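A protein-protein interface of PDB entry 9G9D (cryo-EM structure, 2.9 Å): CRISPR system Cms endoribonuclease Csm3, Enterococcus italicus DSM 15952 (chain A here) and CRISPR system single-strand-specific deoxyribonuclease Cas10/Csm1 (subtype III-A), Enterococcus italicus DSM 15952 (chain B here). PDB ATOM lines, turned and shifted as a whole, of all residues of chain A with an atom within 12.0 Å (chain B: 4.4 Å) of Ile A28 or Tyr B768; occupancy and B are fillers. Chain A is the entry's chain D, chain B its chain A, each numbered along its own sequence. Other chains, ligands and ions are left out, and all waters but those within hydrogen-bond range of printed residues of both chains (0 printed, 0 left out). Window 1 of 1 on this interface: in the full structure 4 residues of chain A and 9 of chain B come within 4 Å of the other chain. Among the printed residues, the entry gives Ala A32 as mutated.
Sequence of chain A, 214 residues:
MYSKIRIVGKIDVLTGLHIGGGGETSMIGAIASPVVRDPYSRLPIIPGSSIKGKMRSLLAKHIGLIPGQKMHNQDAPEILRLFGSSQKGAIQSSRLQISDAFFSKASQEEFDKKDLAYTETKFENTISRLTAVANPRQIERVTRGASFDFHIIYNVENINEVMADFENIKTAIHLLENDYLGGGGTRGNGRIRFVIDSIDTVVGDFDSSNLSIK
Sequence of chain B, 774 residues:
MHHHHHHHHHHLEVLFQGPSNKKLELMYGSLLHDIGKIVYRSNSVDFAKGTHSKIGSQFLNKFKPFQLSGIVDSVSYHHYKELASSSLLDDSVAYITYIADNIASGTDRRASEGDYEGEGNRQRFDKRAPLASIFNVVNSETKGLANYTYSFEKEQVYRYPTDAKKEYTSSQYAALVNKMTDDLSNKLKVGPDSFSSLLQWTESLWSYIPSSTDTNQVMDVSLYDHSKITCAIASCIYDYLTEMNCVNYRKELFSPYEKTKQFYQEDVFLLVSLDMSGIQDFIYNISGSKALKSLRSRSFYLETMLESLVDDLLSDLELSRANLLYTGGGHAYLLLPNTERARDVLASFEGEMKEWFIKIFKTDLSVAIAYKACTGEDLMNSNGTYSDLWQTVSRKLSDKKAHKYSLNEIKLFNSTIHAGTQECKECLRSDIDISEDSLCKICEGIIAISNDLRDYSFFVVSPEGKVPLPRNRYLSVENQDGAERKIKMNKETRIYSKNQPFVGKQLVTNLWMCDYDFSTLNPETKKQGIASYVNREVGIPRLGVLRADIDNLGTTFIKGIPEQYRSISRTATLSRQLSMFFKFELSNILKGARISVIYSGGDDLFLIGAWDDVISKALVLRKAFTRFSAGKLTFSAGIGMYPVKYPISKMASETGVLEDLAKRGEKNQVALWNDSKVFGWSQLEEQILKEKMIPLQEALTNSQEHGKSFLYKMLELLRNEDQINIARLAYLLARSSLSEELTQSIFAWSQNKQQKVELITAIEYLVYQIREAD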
ATOM      1  N   SER A  26       3.676 -16.153  28.538  1.00  0.00           N
ATOM      2  CA  SER A  26       3.041 -15.080  29.293  1.00  0.00           C
ATOM      3  C   SER A  26       1.782 -14.586  28.588  1.00  0.00           C
ATOM      4  O   SER A  26       1.314 -15.202  27.631  1.00  0.00           O
ATOM      5  CB  SER A  26       4.017 -13.920  29.500  1.00  0.00           C
ATOM      6  OG  SER A  26       4.389 -13.346  28.260  1.00  0.00           O
ATOM      7  N   MET A  27       1.249 -13.448  29.043  1.00  0.00           N
ATOM      8  CA  MET A  27      -0.013 -12.919  28.458  1.00  0.00           C
ATOM      9  C   MET A  27       0.257 -12.308  27.072  1.00  0.00           C
ATOM     10  O   MET A  27       1.359 -11.755  26.867  1.00  0.00           O
ATOM     11  CB  MET A  27      -0.639 -11.863  29.375  1.00  0.00           C
ATOM     12  CG  MET A  27      -2.155 -11.884  29.401  1.00  0.00           C
ATOM     13  SD  MET A  27      -2.879 -13.216  30.381  1.00  0.00           S
ATOM     14  CE  MET A  27      -2.932 -14.616  29.252  1.00  0.00           C
ATOM     15  N   ILE A  28      -0.717 -12.402  26.165  1.00  0.00           N
ATOM     16  CA  ILE A  28      -0.546 -11.863  24.782  1.00  0.00           C
ATOM     17  C   ILE A  28      -0.395 -10.336  24.845  1.00  0.00           C
ATOM     18  O   ILE A  28      -1.069  -9.707  25.689  1.00  0.00           O
ATOM     19  CB  ILE A  28      -1.726 -12.282  23.884  1.00  0.00           C
ATOM     20  CG1 ILE A  28      -1.512 -11.842  22.443  1.00  0.00           C
ATOM     21  CG2 ILE A  28      -3.063 -11.787  24.436  1.00  0.00           C
ATOM     22  CD1 ILE A  28      -0.478 -12.669  21.704  1.00  0.00           C
ATOM     23  N   GLY A  29       0.488  -9.768  24.020  1.00  0.00           N
ATOM     24  CA  GLY A  29       0.624  -8.300  23.950  1.00  0.00           C
ATOM     25  C   GLY A  29       1.418  -7.759  25.119  1.00  0.00           C
ATOM     26  O   GLY A  29       1.451  -6.523  25.286  1.00  0.00           O
ATOM     27  N   ALA A  30       2.039  -8.640  25.904  1.00  0.00           N
ATOM     28  CA  ALA A  30       2.758  -8.184  27.115  1.00  0.00           C
ATOM     29  C   ALA A  30       4.234  -8.562  27.019  1.00  0.00           C
ATOM     30  O   ALA A  30       4.558  -9.598  26.401  1.00  0.00           O
ATOM     31  CB  ALA A  30       2.121  -8.783  28.347  1.00  0.00           C
ATOM     32  N   ILE A  31       5.101  -7.742  27.614  1.00  0.00           N
ATOM     33  CA  ILE A  31       6.556  -8.063  27.638  1.00  0.00           C
ATOM     34  C   ILE A  31       6.687  -9.529  28.047  1.00  0.00           C
ATOM     35  O   ILE A  31       6.247  -9.882  29.161  1.00  0.00           O
ATOM     36  CB  ILE A  31       7.287  -7.158  28.645  1.00  0.00           C
ATOM     37  CG1 ILE A  31       6.985  -5.684  28.400  1.00  0.00           C
ATOM     38  CG2 ILE A  31       8.792  -7.437  28.659  1.00  0.00           C
ATOM     39  CD1 ILE A  31       6.047  -5.064  29.419  1.00  0.00           C
ATOM     40  N   ALA A  32       7.270 -10.336  27.173  1.00  0.00           N
ATOM     41  CA  ALA A  32       7.415 -11.754  27.467  1.00  0.00           C
ATOM     42  C   ALA A  32       8.763 -12.096  28.085  1.00  0.00           C
ATOM     43  O   ALA A  32       9.030 -13.273  28.345  1.00  0.00           O
ATOM     44  CB  ALA A  32       7.199 -12.580  26.198  1.00  0.00           C
ATOM     45  N   SER A  33       9.614 -11.104  28.329  1.00  0.00           N
ATOM     46  CA  SER A  33      10.964 -11.325  28.845  1.00  0.00           C
ATOM     47  C   SER A  33      11.202 -10.440  30.062  1.00  0.00           C
ATOM     48  O   SER A  33      11.959  -9.465  30.000  1.00  0.00           O
ATOM     49  CB  SER A  33      12.007 -11.057  27.759  1.00  0.00           C
ATOM     50  OG  SER A  33      11.799 -11.896  26.638  1.00  0.00           O
ATOM     51  N   PRO A  34      10.568 -10.753  31.193  1.00  0.00           N
ATOM     52  CA  PRO A  34      10.777  -9.941  32.395  1.00  0.00           C
ATOM     53  C   PRO A  34      12.153 -10.171  32.990  1.00  0.00           C
ATOM     54  O   PRO A  34      12.677 -11.286  32.976  1.00  0.00           O
ATOM     55  CB  PRO A  34       9.671 -10.419  33.340  1.00  0.00           C
ATOM     56  CG  PRO A  34       9.436 -11.823  32.934  1.00  0.00           C
ATOM     57  CD  PRO A  34       9.647 -11.875  31.443  1.00  0.00           C
ATOM     58  N   THR A 121      11.087  -0.798  28.753  1.00  0.00           N
ATOM     59  CA  THR A 121      10.782  -1.948  27.872  1.00  0.00           C
ATOM     60  C   THR A 121      11.289  -1.619  26.481  1.00  0.00           C
ATOM     61  O   THR A 121      11.074  -0.470  26.046  1.00  0.00           O
ATOM     62  CB  THR A 121       9.282  -2.228  27.878  1.00  0.00           C
ATOM     63  OG1 THR A 121       9.030  -2.804  29.155  1.00  0.00           O
ATOM     64  CG2 THR A 121       8.863  -3.192  26.784  1.00  0.00           C
ATOM     65  N   PHE A 123      11.287  -2.490  22.398  1.00  0.00           N
ATOM     66  CA  PHE A 123      10.551  -3.231  21.342  1.00  0.00           C
ATOM     67  C   PHE A 123      11.552  -3.595  20.261  1.00  0.00           C
ATOM     68  O   PHE A 123      12.267  -2.697  19.773  1.00  0.00           O
ATOM     69  CB  PHE A 123       9.387  -2.406  20.788  1.00  0.00           C
ATOM     70  CG  PHE A 123       8.136  -2.351  21.654  1.00  0.00           C
ATOM     71  CD1 PHE A 123       8.219  -2.310  23.042  1.00  0.00           C
ATOM     72  CD2 PHE A 123       6.874  -2.359  21.074  1.00  0.00           C
ATOM     73  CE1 PHE A 123       7.074  -2.260  23.819  1.00  0.00           C
ATOM     74  CE2 PHE A 123       5.731  -2.313  21.857  1.00  0.00           C
ATOM     75  CZ  PHE A 123       5.834  -2.264  23.227  1.00  0.00           C
ATOM     76  N   ASN A 135       9.095 -10.282  13.157  1.00  0.00           N
ATOM     77  CA  ASN A 135       8.464 -10.833  14.384  1.00  0.00           C
ATOM     78  C   ASN A 135       8.834  -9.918  15.548  1.00  0.00           C
ATOM     79  O   ASN A 135      10.039  -9.717  15.768  1.00  0.00           O
ATOM     80  CB  ASN A 135       8.905 -12.272  14.611  1.00  0.00           C
ATOM     81  CG  ASN A 135       8.130 -12.952  15.710  1.00  0.00           C
ATOM     82  OD1 ASN A 135       8.728 -13.441  16.674  1.00  0.00           O
ATOM     83  ND2 ASN A 135       6.814 -13.019  15.577  1.00  0.00           N
ATOM     84  N   PRO A 136       7.866  -9.415  16.342  1.00  0.00           N
ATOM     85  CA  PRO A 136       8.172  -8.445  17.382  1.00  0.00           C
ATOM     86  C   PRO A 136       8.299  -8.974  18.800  1.00  0.00           C
ATOM     87  O   PRO A 136       7.431  -9.723  19.287  1.00  0.00           O
ATOM     88  CB  PRO A 136       6.959  -7.523  17.229  1.00  0.00           C
ATOM     89  CG  PRO A 136       5.832  -8.429  16.792  1.00  0.00           C
ATOM     90  CD  PRO A 136       6.453  -9.686  16.213  1.00  0.00           C
ATOM     91  N   ARG A 137       9.396  -8.607  19.456  1.00  0.00           N
ATOM     92  CA  ARG A 137       9.624  -9.041  20.854  1.00  0.00           C
ATOM     93  C   ARG A 137       9.739  -7.818  21.772  1.00  0.00           C
ATOM     94  O   ARG A 137      10.454  -6.865  21.405  1.00  0.00           O
ATOM     95  CB  ARG A 137      10.912  -9.862  20.935  1.00  0.00           C
ATOM     96  CG  ARG A 137      12.103  -9.266  20.203  1.00  0.00           C
ATOM     97  CD  ARG A 137      13.373 -10.056  20.448  1.00  0.00           C
ATOM     98  NE  ARG A 137      14.538  -9.543  19.719  1.00  0.00           N
ATOM     99  CZ  ARG A 137      14.661  -9.479  18.399  1.00  0.00           C
ATOM    100  NH1 ARG A 137      13.740 -10.009  17.616  1.00  0.00           N
ATOM    101  NH2 ARG A 137      15.716  -8.891  17.866  1.00  0.00           N
ATOM    102  N   GLN A 138       9.047  -7.831  22.912  1.00  0.00           N
ATOM    103  CA  GLN A 138       9.206  -6.731  23.896  1.00  0.00           C
ATOM    104  C   GLN A 138      10.071  -7.267  25.039  1.00  0.00           C
ATOM    105  O   GLN A 138       9.684  -8.290  25.633  1.00  0.00           O
ATOM    106  CB  GLN A 138       7.871  -6.250  24.461  1.00  0.00           C
ATOM    107  CG  GLN A 138       6.776  -6.059  23.421  1.00  0.00           C
ATOM    108  CD  GLN A 138       5.448  -5.685  24.040  1.00  0.00           C
ATOM    109  OE1 GLN A 138       5.332  -5.520  25.260  1.00  0.00           O
ATOM    110  NE2 GLN A 138       4.431  -5.542  23.203  1.00  0.00           N
ATOM    111  N   GLY B 539      -4.490 -21.203  15.571  1.00  0.00           N
ATOM    112  CA  GLY B 539      -4.420 -21.004  17.002  1.00  0.00           C
ATOM    113  C   GLY B 539      -3.004 -21.132  17.533  1.00  0.00           C
ATOM    114  O   GLY B 539      -2.122 -21.723  16.914  1.00  0.00           O
ATOM    115  N   ILE B 540      -2.791 -20.553  18.710  1.00  0.00           N
ATOM    116  CA  ILE B 540      -1.441 -20.580  19.281  1.00  0.00           C
ATOM    117  C   ILE B 540      -1.117 -21.997  19.734  1.00  0.00           C
ATOM    118  O   ILE B 540      -1.970 -22.658  20.362  1.00  0.00           O
ATOM    119  CB  ILE B 540      -1.321 -19.578  20.444  1.00  0.00           C
ATOM    120  CG1 ILE B 540       0.088 -19.607  21.036  1.00  0.00           C
ATOM    121  CG2 ILE B 540      -2.367 -19.852  21.512  1.00  0.00           C
ATOM    122  CD1 ILE B 540       0.323 -18.556  22.092  1.00  0.00           C
ATOM    123  N   TRP B 611      -4.685 -25.975  25.024  1.00  0.00           N
ATOM    124  CA  TRP B 611      -5.234 -24.848  25.772  1.00  0.00           C
ATOM    125  C   TRP B 611      -6.697 -24.616  25.422  1.00  0.00           C
ATOM    126  O   TRP B 611      -7.494 -24.213  26.277  1.00  0.00           O
ATOM    127  CB  TRP B 611      -4.415 -23.585  25.495  1.00  0.00           C
ATOM    128  CG  TRP B 611      -4.630 -23.038  24.121  1.00  0.00           C
ATOM    129  CD1 TRP B 611      -3.969 -23.394  22.987  1.00  0.00           C
ATOM    130  CD2 TRP B 611      -5.590 -22.047  23.734  1.00  0.00           C
ATOM    131  NE1 TRP B 611      -4.450 -22.683  21.916  1.00  0.00           N
ATOM    132  CE2 TRP B 611      -5.448 -21.849  22.349  1.00  0.00           C
ATOM    133  CE3 TRP B 611      -6.553 -21.308  24.425  1.00  0.00           C
ATOM    134  CZ2 TRP B 611      -6.231 -20.944  21.641  1.00  0.00           C
ATOM    135  CZ3 TRP B 611      -7.329 -20.411  23.722  1.00  0.00           C
ATOM    136  CH2 TRP B 611      -7.165 -20.237  22.345  1.00  0.00           C
ATOM    137  N   MET B 641      -1.569 -21.882  30.843  1.00  0.00           N
ATOM    138  CA  MET B 641      -1.200 -22.018  29.441  1.00  0.00           C
ATOM    139  C   MET B 641       0.317 -22.039  29.326  1.00  0.00           C
ATOM    140  O   MET B 641       0.990 -21.107  29.777  1.00  0.00           O
ATOM    141  CB  MET B 641      -1.789 -20.875  28.611  1.00  0.00           C
ATOM    142  CG  MET B 641      -1.201 -20.745  27.223  1.00  0.00           C
ATOM    143  SD  MET B 641      -1.919 -19.376  26.302  1.00  0.00           S
ATOM    144  CE  MET B 641      -3.570 -20.001  26.024  1.00  0.00           C
ATOM    145  N   TRP B 673      -5.455 -18.827  33.066  1.00  0.00           N
ATOM    146  CA  TRP B 673      -4.227 -18.142  32.592  1.00  0.00           C
ATOM    147  C   TRP B 673      -3.639 -17.369  33.767  1.00  0.00           C
ATOM    148  O   TRP B 673      -3.373 -17.984  34.813  1.00  0.00           O
ATOM    149  CB  TRP B 673      -4.506 -17.236  31.384  1.00  0.00           C
ATOM    150  CG  TRP B 673      -5.135 -17.941  30.213  1.00  0.00           C
ATOM    151  CD1 TRP B 673      -5.048 -19.265  29.900  1.00  0.00           C
ATOM    152  CD2 TRP B 673      -5.939 -17.336  29.178  1.00  0.00           C
ATOM    153  NE1 TRP B 673      -5.751 -19.530  28.754  1.00  0.00           N
ATOM    154  CE2 TRP B 673      -6.304 -18.367  28.287  1.00  0.00           C
ATOM    155  CE3 TRP B 673      -6.384 -16.034  28.923  1.00  0.00           C
ATOM    156  CZ2 TRP B 673      -7.092 -18.131  27.163  1.00  0.00           C
ATOM    157  CZ3 TRP B 673      -7.160 -15.803  27.809  1.00  0.00           C
ATOM    158  CH2 TRP B 673      -7.506 -16.838  26.944  1.00  0.00           C
ATOM    159  N   TYR B 712      -5.467  -5.559  18.842  1.00  0.00           N
ATOM    160  CA  TYR B 712      -4.332  -5.163  19.718  1.00  0.00           C
ATOM    161  C   TYR B 712      -4.476  -3.692  20.117  1.00  0.00           C
ATOM    162  O   TYR B 712      -4.178  -3.352  21.279  1.00  0.00           O
ATOM    163  CB  TYR B 712      -3.009  -5.462  19.009  1.00  0.00           C
ATOM    164  CG  TYR B 712      -2.568  -6.919  19.047  1.00  0.00           C
ATOM    165  CD1 TYR B 712      -3.050  -7.837  18.125  1.00  0.00           C
ATOM    166  CD2 TYR B 712      -1.651  -7.371  19.988  1.00  0.00           C
ATOM    167  CE1 TYR B 712      -2.647  -9.160  18.141  1.00  0.00           C
ATOM    168  CE2 TYR B 712      -1.238  -8.693  20.015  1.00  0.00           C
ATOM    169  CZ  TYR B 712      -1.736  -9.588  19.087  1.00  0.00           C
ATOM    170  OH  TYR B 712      -1.339 -10.892  19.090  1.00  0.00           O
ATOM    171  N   ARG B 719      -6.837  -2.078  29.710  1.00  0.00           N
ATOM    172  CA  ARG B 719      -5.633  -2.403  30.523  1.00  0.00           C
ATOM    173  C   ARG B 719      -4.934  -1.076  30.864  1.00  0.00           C
ATOM    174  O   ARG B 719      -3.758  -1.120  31.282  1.00  0.00           O
ATOM    175  CB  ARG B 719      -4.612  -3.331  29.850  1.00  0.00           C
ATOM    176  CG  ARG B 719      -5.068  -4.639  29.218  1.00  0.00           C
ATOM    177  CD  ARG B 719      -3.939  -5.164  28.344  1.00  0.00           C
ATOM    178  NE  ARG B 719      -4.071  -6.562  27.923  1.00  0.00           N
ATOM    179  CZ  ARG B 719      -3.174  -7.192  27.173  1.00  0.00           C
ATOM    180  NH1 ARG B 719      -3.227  -8.504  27.030  1.00  0.00           N
ATOM    181  NH2 ARG B 719      -2.220  -6.506  26.569  1.00  0.00           N
ATOM    182  N   GLU B 764      -8.260 -11.521  24.202  1.00  0.00           N
ATOM    183  CA  GLU B 764      -7.116 -12.457  24.352  1.00  0.00           C
ATOM    184  C   GLU B 764      -7.501 -13.843  23.804  1.00  0.00           C
ATOM    185  O   GLU B 764      -6.747 -14.372  22.967  1.00  0.00           O
ATOM    186  CB  GLU B 764      -6.684 -12.513  25.814  1.00  0.00           C
ATOM    187  CG  GLU B 764      -6.307 -11.144  26.366  1.00  0.00           C
ATOM    188  CD  GLU B 764      -5.275 -11.276  27.463  1.00  0.00           C
ATOM    189  OE1 GLU B 764      -4.885 -12.431  27.724  1.00  0.00           O
ATOM    190  OE2 GLU B 764      -4.865 -10.252  28.045  1.00  0.00           O
ATOM    191  N   TYR B 765      -8.622 -14.408  24.263  1.00  0.00           N
ATOM    192  CA  TYR B 765      -9.020 -15.729  23.791  1.00  0.00           C
ATOM    193  C   TYR B 765      -9.138 -15.746  22.275  1.00  0.00           C
ATOM    194  O   TYR B 765      -8.697 -16.697  21.620  1.00  0.00           O
ATOM    195  CB  TYR B 765     -10.342 -16.145  24.436  1.00  0.00           C
ATOM    196  CG  TYR B 765     -10.583 -17.639  24.437  1.00  0.00           C
ATOM    197  CD1 TYR B 765     -10.967 -18.304  23.280  1.00  0.00           C
ATOM    198  CD2 TYR B 765     -10.433 -18.381  25.598  1.00  0.00           C
ATOM    199  CE1 TYR B 765     -11.190 -19.666  23.279  1.00  0.00           C
ATOM    200  CE2 TYR B 765     -10.654 -19.743  25.606  1.00  0.00           C
ATOM    201  CZ  TYR B 765     -11.033 -20.381  24.445  1.00  0.00           C
ATOM    202  OH  TYR B 765     -11.254 -21.737  24.448  1.00  0.00           O
ATOM    203  N   LEU B 766      -9.725 -14.695  21.700  1.00  0.00           N
ATOM    204  CA  LEU B 766      -9.828 -14.604  20.248  1.00  0.00           C
ATOM    205  C   LEU B 766      -8.453 -14.474  19.604  1.00  0.00           C
ATOM    206  O   LEU B 766      -8.202 -15.056  18.544  1.00  0.00           O
ATOM    207  CB  LEU B 766     -10.720 -13.425  19.866  1.00  0.00           C
ATOM    208  CG  LEU B 766     -10.806 -13.053  18.389  1.00  0.00           C
ATOM    209  CD1 LEU B 766     -11.250 -14.242  17.559  1.00  0.00           C
ATOM    210  CD2 LEU B 766     -11.759 -11.886  18.211  1.00  0.00           C
ATOM    211  N   VAL B 767      -7.553 -13.710  20.225  1.00  0.00           N
ATOM    212  CA  VAL B 767      -6.206 -13.560  19.679  1.00  0.00           C
ATOM    213  C   VAL B 767      -5.463 -14.888  19.718  1.00  0.00           C
ATOM    214  O   VAL B 767      -4.809 -15.280  18.744  1.00  0.00           O
ATOM    215  CB  VAL B 767      -5.440 -12.458  20.434  1.00  0.00           C
ATOM    216  CG1 VAL B 767      -3.972 -12.508  20.076  1.00  0.00           C
ATOM    217  CG2 VAL B 767      -6.011 -11.094  20.099  1.00  0.00           C
ATOM    218  N   TYR B 768      -5.547 -15.599  20.844  1.00  0.00           N
ATOM    219  CA  TYR B 768      -4.920 -16.913  20.942  1.00  0.00           C
ATOM    220  C   TYR B 768      -5.526 -17.890  19.944  1.00  0.00           C
ATOM    221  O   TYR B 768      -4.812 -18.699  19.341  1.00  0.00           O
ATOM    222  CB  TYR B 768      -5.066 -17.457  22.361  1.00  0.00           C
ATOM    223  CG  TYR B 768      -4.096 -16.878  23.358  1.00  0.00           C
ATOM    224  CD1 TYR B 768      -2.812 -16.521  22.980  1.00  0.00           C
ATOM    225  CD2 TYR B 768      -4.464 -16.696  24.682  1.00  0.00           C
ATOM    226  CE1 TYR B 768      -1.923 -15.997  23.892  1.00  0.00           C
ATOM    227  CE2 TYR B 768      -3.583 -16.173  25.600  1.00  0.00           C
ATOM    228  CZ  TYR B 768      -2.313 -15.824  25.200  1.00  0.00           C
ATOM    229  OH  TYR B 768      -1.426 -15.300  26.110  1.00  0.00           O
ATOM    230  N   GLN B 769      -6.846 -17.835  19.762  1.00  0.00           N
ATOM    231  CA  GLN B 769      -7.529 -18.819  18.930  1.00  0.00           C
ATOM    232  C   GLN B 769      -7.260 -18.586  17.448  1.00  0.00           C
ATOM    233  O   GLN B 769      -7.454 -19.490  16.627  1.00  0.00           O
ATOM    234  CB  GLN B 769      -9.029 -18.786  19.215  1.00  0.00           C
ATOM    235  CG  GLN B 769      -9.782 -20.016  18.749  1.00  0.00           C
ATOM    236  CD  GLN B 769     -11.215 -20.033  19.236  1.00  0.00           C
ATOM    237  OE1 GLN B 769     -11.661 -19.106  19.910  1.00  0.00           O
ATOM    238  NE2 GLN B 769     -11.943 -21.091  18.902  1.00  0.00           N
ATOM    239  N   ILE B 770      -6.814 -17.380  17.083  1.00  0.00           N
ATOM    240  CA  ILE B 770      -6.706 -17.012  15.675  1.00  0.00           C
ATOM    241  C   ILE B 770      -5.261 -16.887  15.206  1.00  0.00           C
ATOM    242  O   ILE B 770      -5.026 -16.536  14.041  1.00  0.00           O
ATOM    243  CB  ILE B 770      -7.492 -15.705  15.429  1.00  0.00           C
ATOM    244  CG1 ILE B 770      -8.004 -15.640  13.988  1.00  0.00           C
ATOM    245  CG2 ILE B 770      -6.648 -14.484  15.785  1.00  0.00           C
ATOM    246  CD1 ILE B 770      -9.008 -14.535  13.757  1.00  0.00           C
ATOM    247  N   ARG B 771      -4.287 -17.181  16.065  1.00  0.00           N
ATOM    248  CA  ARG B 771      -2.887 -17.102  15.668  1.00  0.00           C
ATOM    249  C   ARG B 771      -2.581 -18.075  14.537  1.00  0.00           C
ATOM    250  O   ARG B 771      -3.091 -19.198  14.508  1.00  0.00           O
ATOM    251  CB  ARG B 771      -1.984 -17.399  16.866  1.00  0.00           C
ATOM    252  CG  ARG B 771      -1.802 -16.228  17.806  1.00  0.00           C
ATOM    253  CD  ARG B 771      -0.615 -15.383  17.397  1.00  0.00           C
ATOM    254  NE  ARG B 771       0.646 -16.036  17.725  1.00  0.00           N
ATOM    255  CZ  ARG B 771       1.313 -15.848  18.856  1.00  0.00           C
ATOM    256  NH1 ARG B 771       0.863 -15.031  19.793  1.00  0.00           N
ATOM    257  NH2 ARG B 771       2.459 -16.491  19.048  1.00  0.00           N
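Of the 15 printed residues of chain A, 4 touch a printed residue of chain B. Hydrophobic or aromatic side chains of chain A that line the printed part of chain B: Met A27 and Ile A28. Among the printed residues, 11 pairs touch across the chains. Among the printed residues, no Asp or Glu carboxylate lies within 4 Å of a Lys or Arg side-chain nitrogen of the other chain.
Of the printed residues of chain B, Met A27 touches Trp B673 (3.7 Å), Glu B764 (3.3 Å) and Tyr B768 (3.6 Å). Of chain B, only Tyr B712 (3.3 Å), Arg B719 (2.8 Å), Glu B764 (3.8 Å), Val B767 (3.5 Å), Tyr B768 (3.0 Å) and Arg B771 (3.3 Å) come within 4 Å of Ile A28. No residue of chain A comes within 4 Å of Ile B540. Of the printed residues of chain A, Trp B673 touches Met A27. Of the printed residues of chain A, Arg B719 touches Ile A28 and Gly A29. Glu B764 touches just these residues of chain A: Met A27 and Ile A28. No residue of chain A comes within 4 Å of Tyr B765. Val B767 touches just one residue of chain A: Ile A28. Of chain A, only Ser A26 (3.1 Å), Met A27 (3.6 Å) and Ile A28 (3.0 Å) come within 4 Å of Tyr B768. Gln B769 touches none of the printed residues of chain A. Arg B771 touches just one residue of chain A: Ile A28 (3.3 Å). The nearest printed residue of chain B that does not touch Met A27 is Arg B719 (4.3 Å).
The backbone carbonyl oxygen (O) of Ser A26 sits at hydrogen-bond distance from the side-chain hydroxyl (OH) of Tyr B768. NH1 of Arg B719 is in hydrogen-bond range of O of Ile A28 (2.8 Å). The backbone NH of Ile A28 is in hydrogen-bond range of the side-chain hydroxyl of Tyr B768 (3.0 Å). SD of Met A27 lies close to OE1 of Glu B764, at 3.4 Å.
Among the printed residues, merely in contact across the chains: Met A27 with Trp B673 (3.7 Å), Met A27 with Tyr B768 (3.6 Å), Ile A28 with Tyr B712 (3.3 Å), Ile A28 with Glu B764 (3.8 Å), Ile A28 with Val B767 (3.5 Å), Ile A28 with Arg B771 (3.3 Å) and Gly A29 with Arg B719 (3.9 Å).
The backbone NH (N) of Gly B539 sits at hydrogen-bond distance from the backbone carbonyl oxygen (O) of Arg B771, at 2.7 Å. N of Ile B540 sits at hydrogen-bond distance from O of Tyr B768 (2.8 Å). NH1 of Arg B719 is in salt-bridge range of OE2 of Glu B764, 2.6 Å away.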
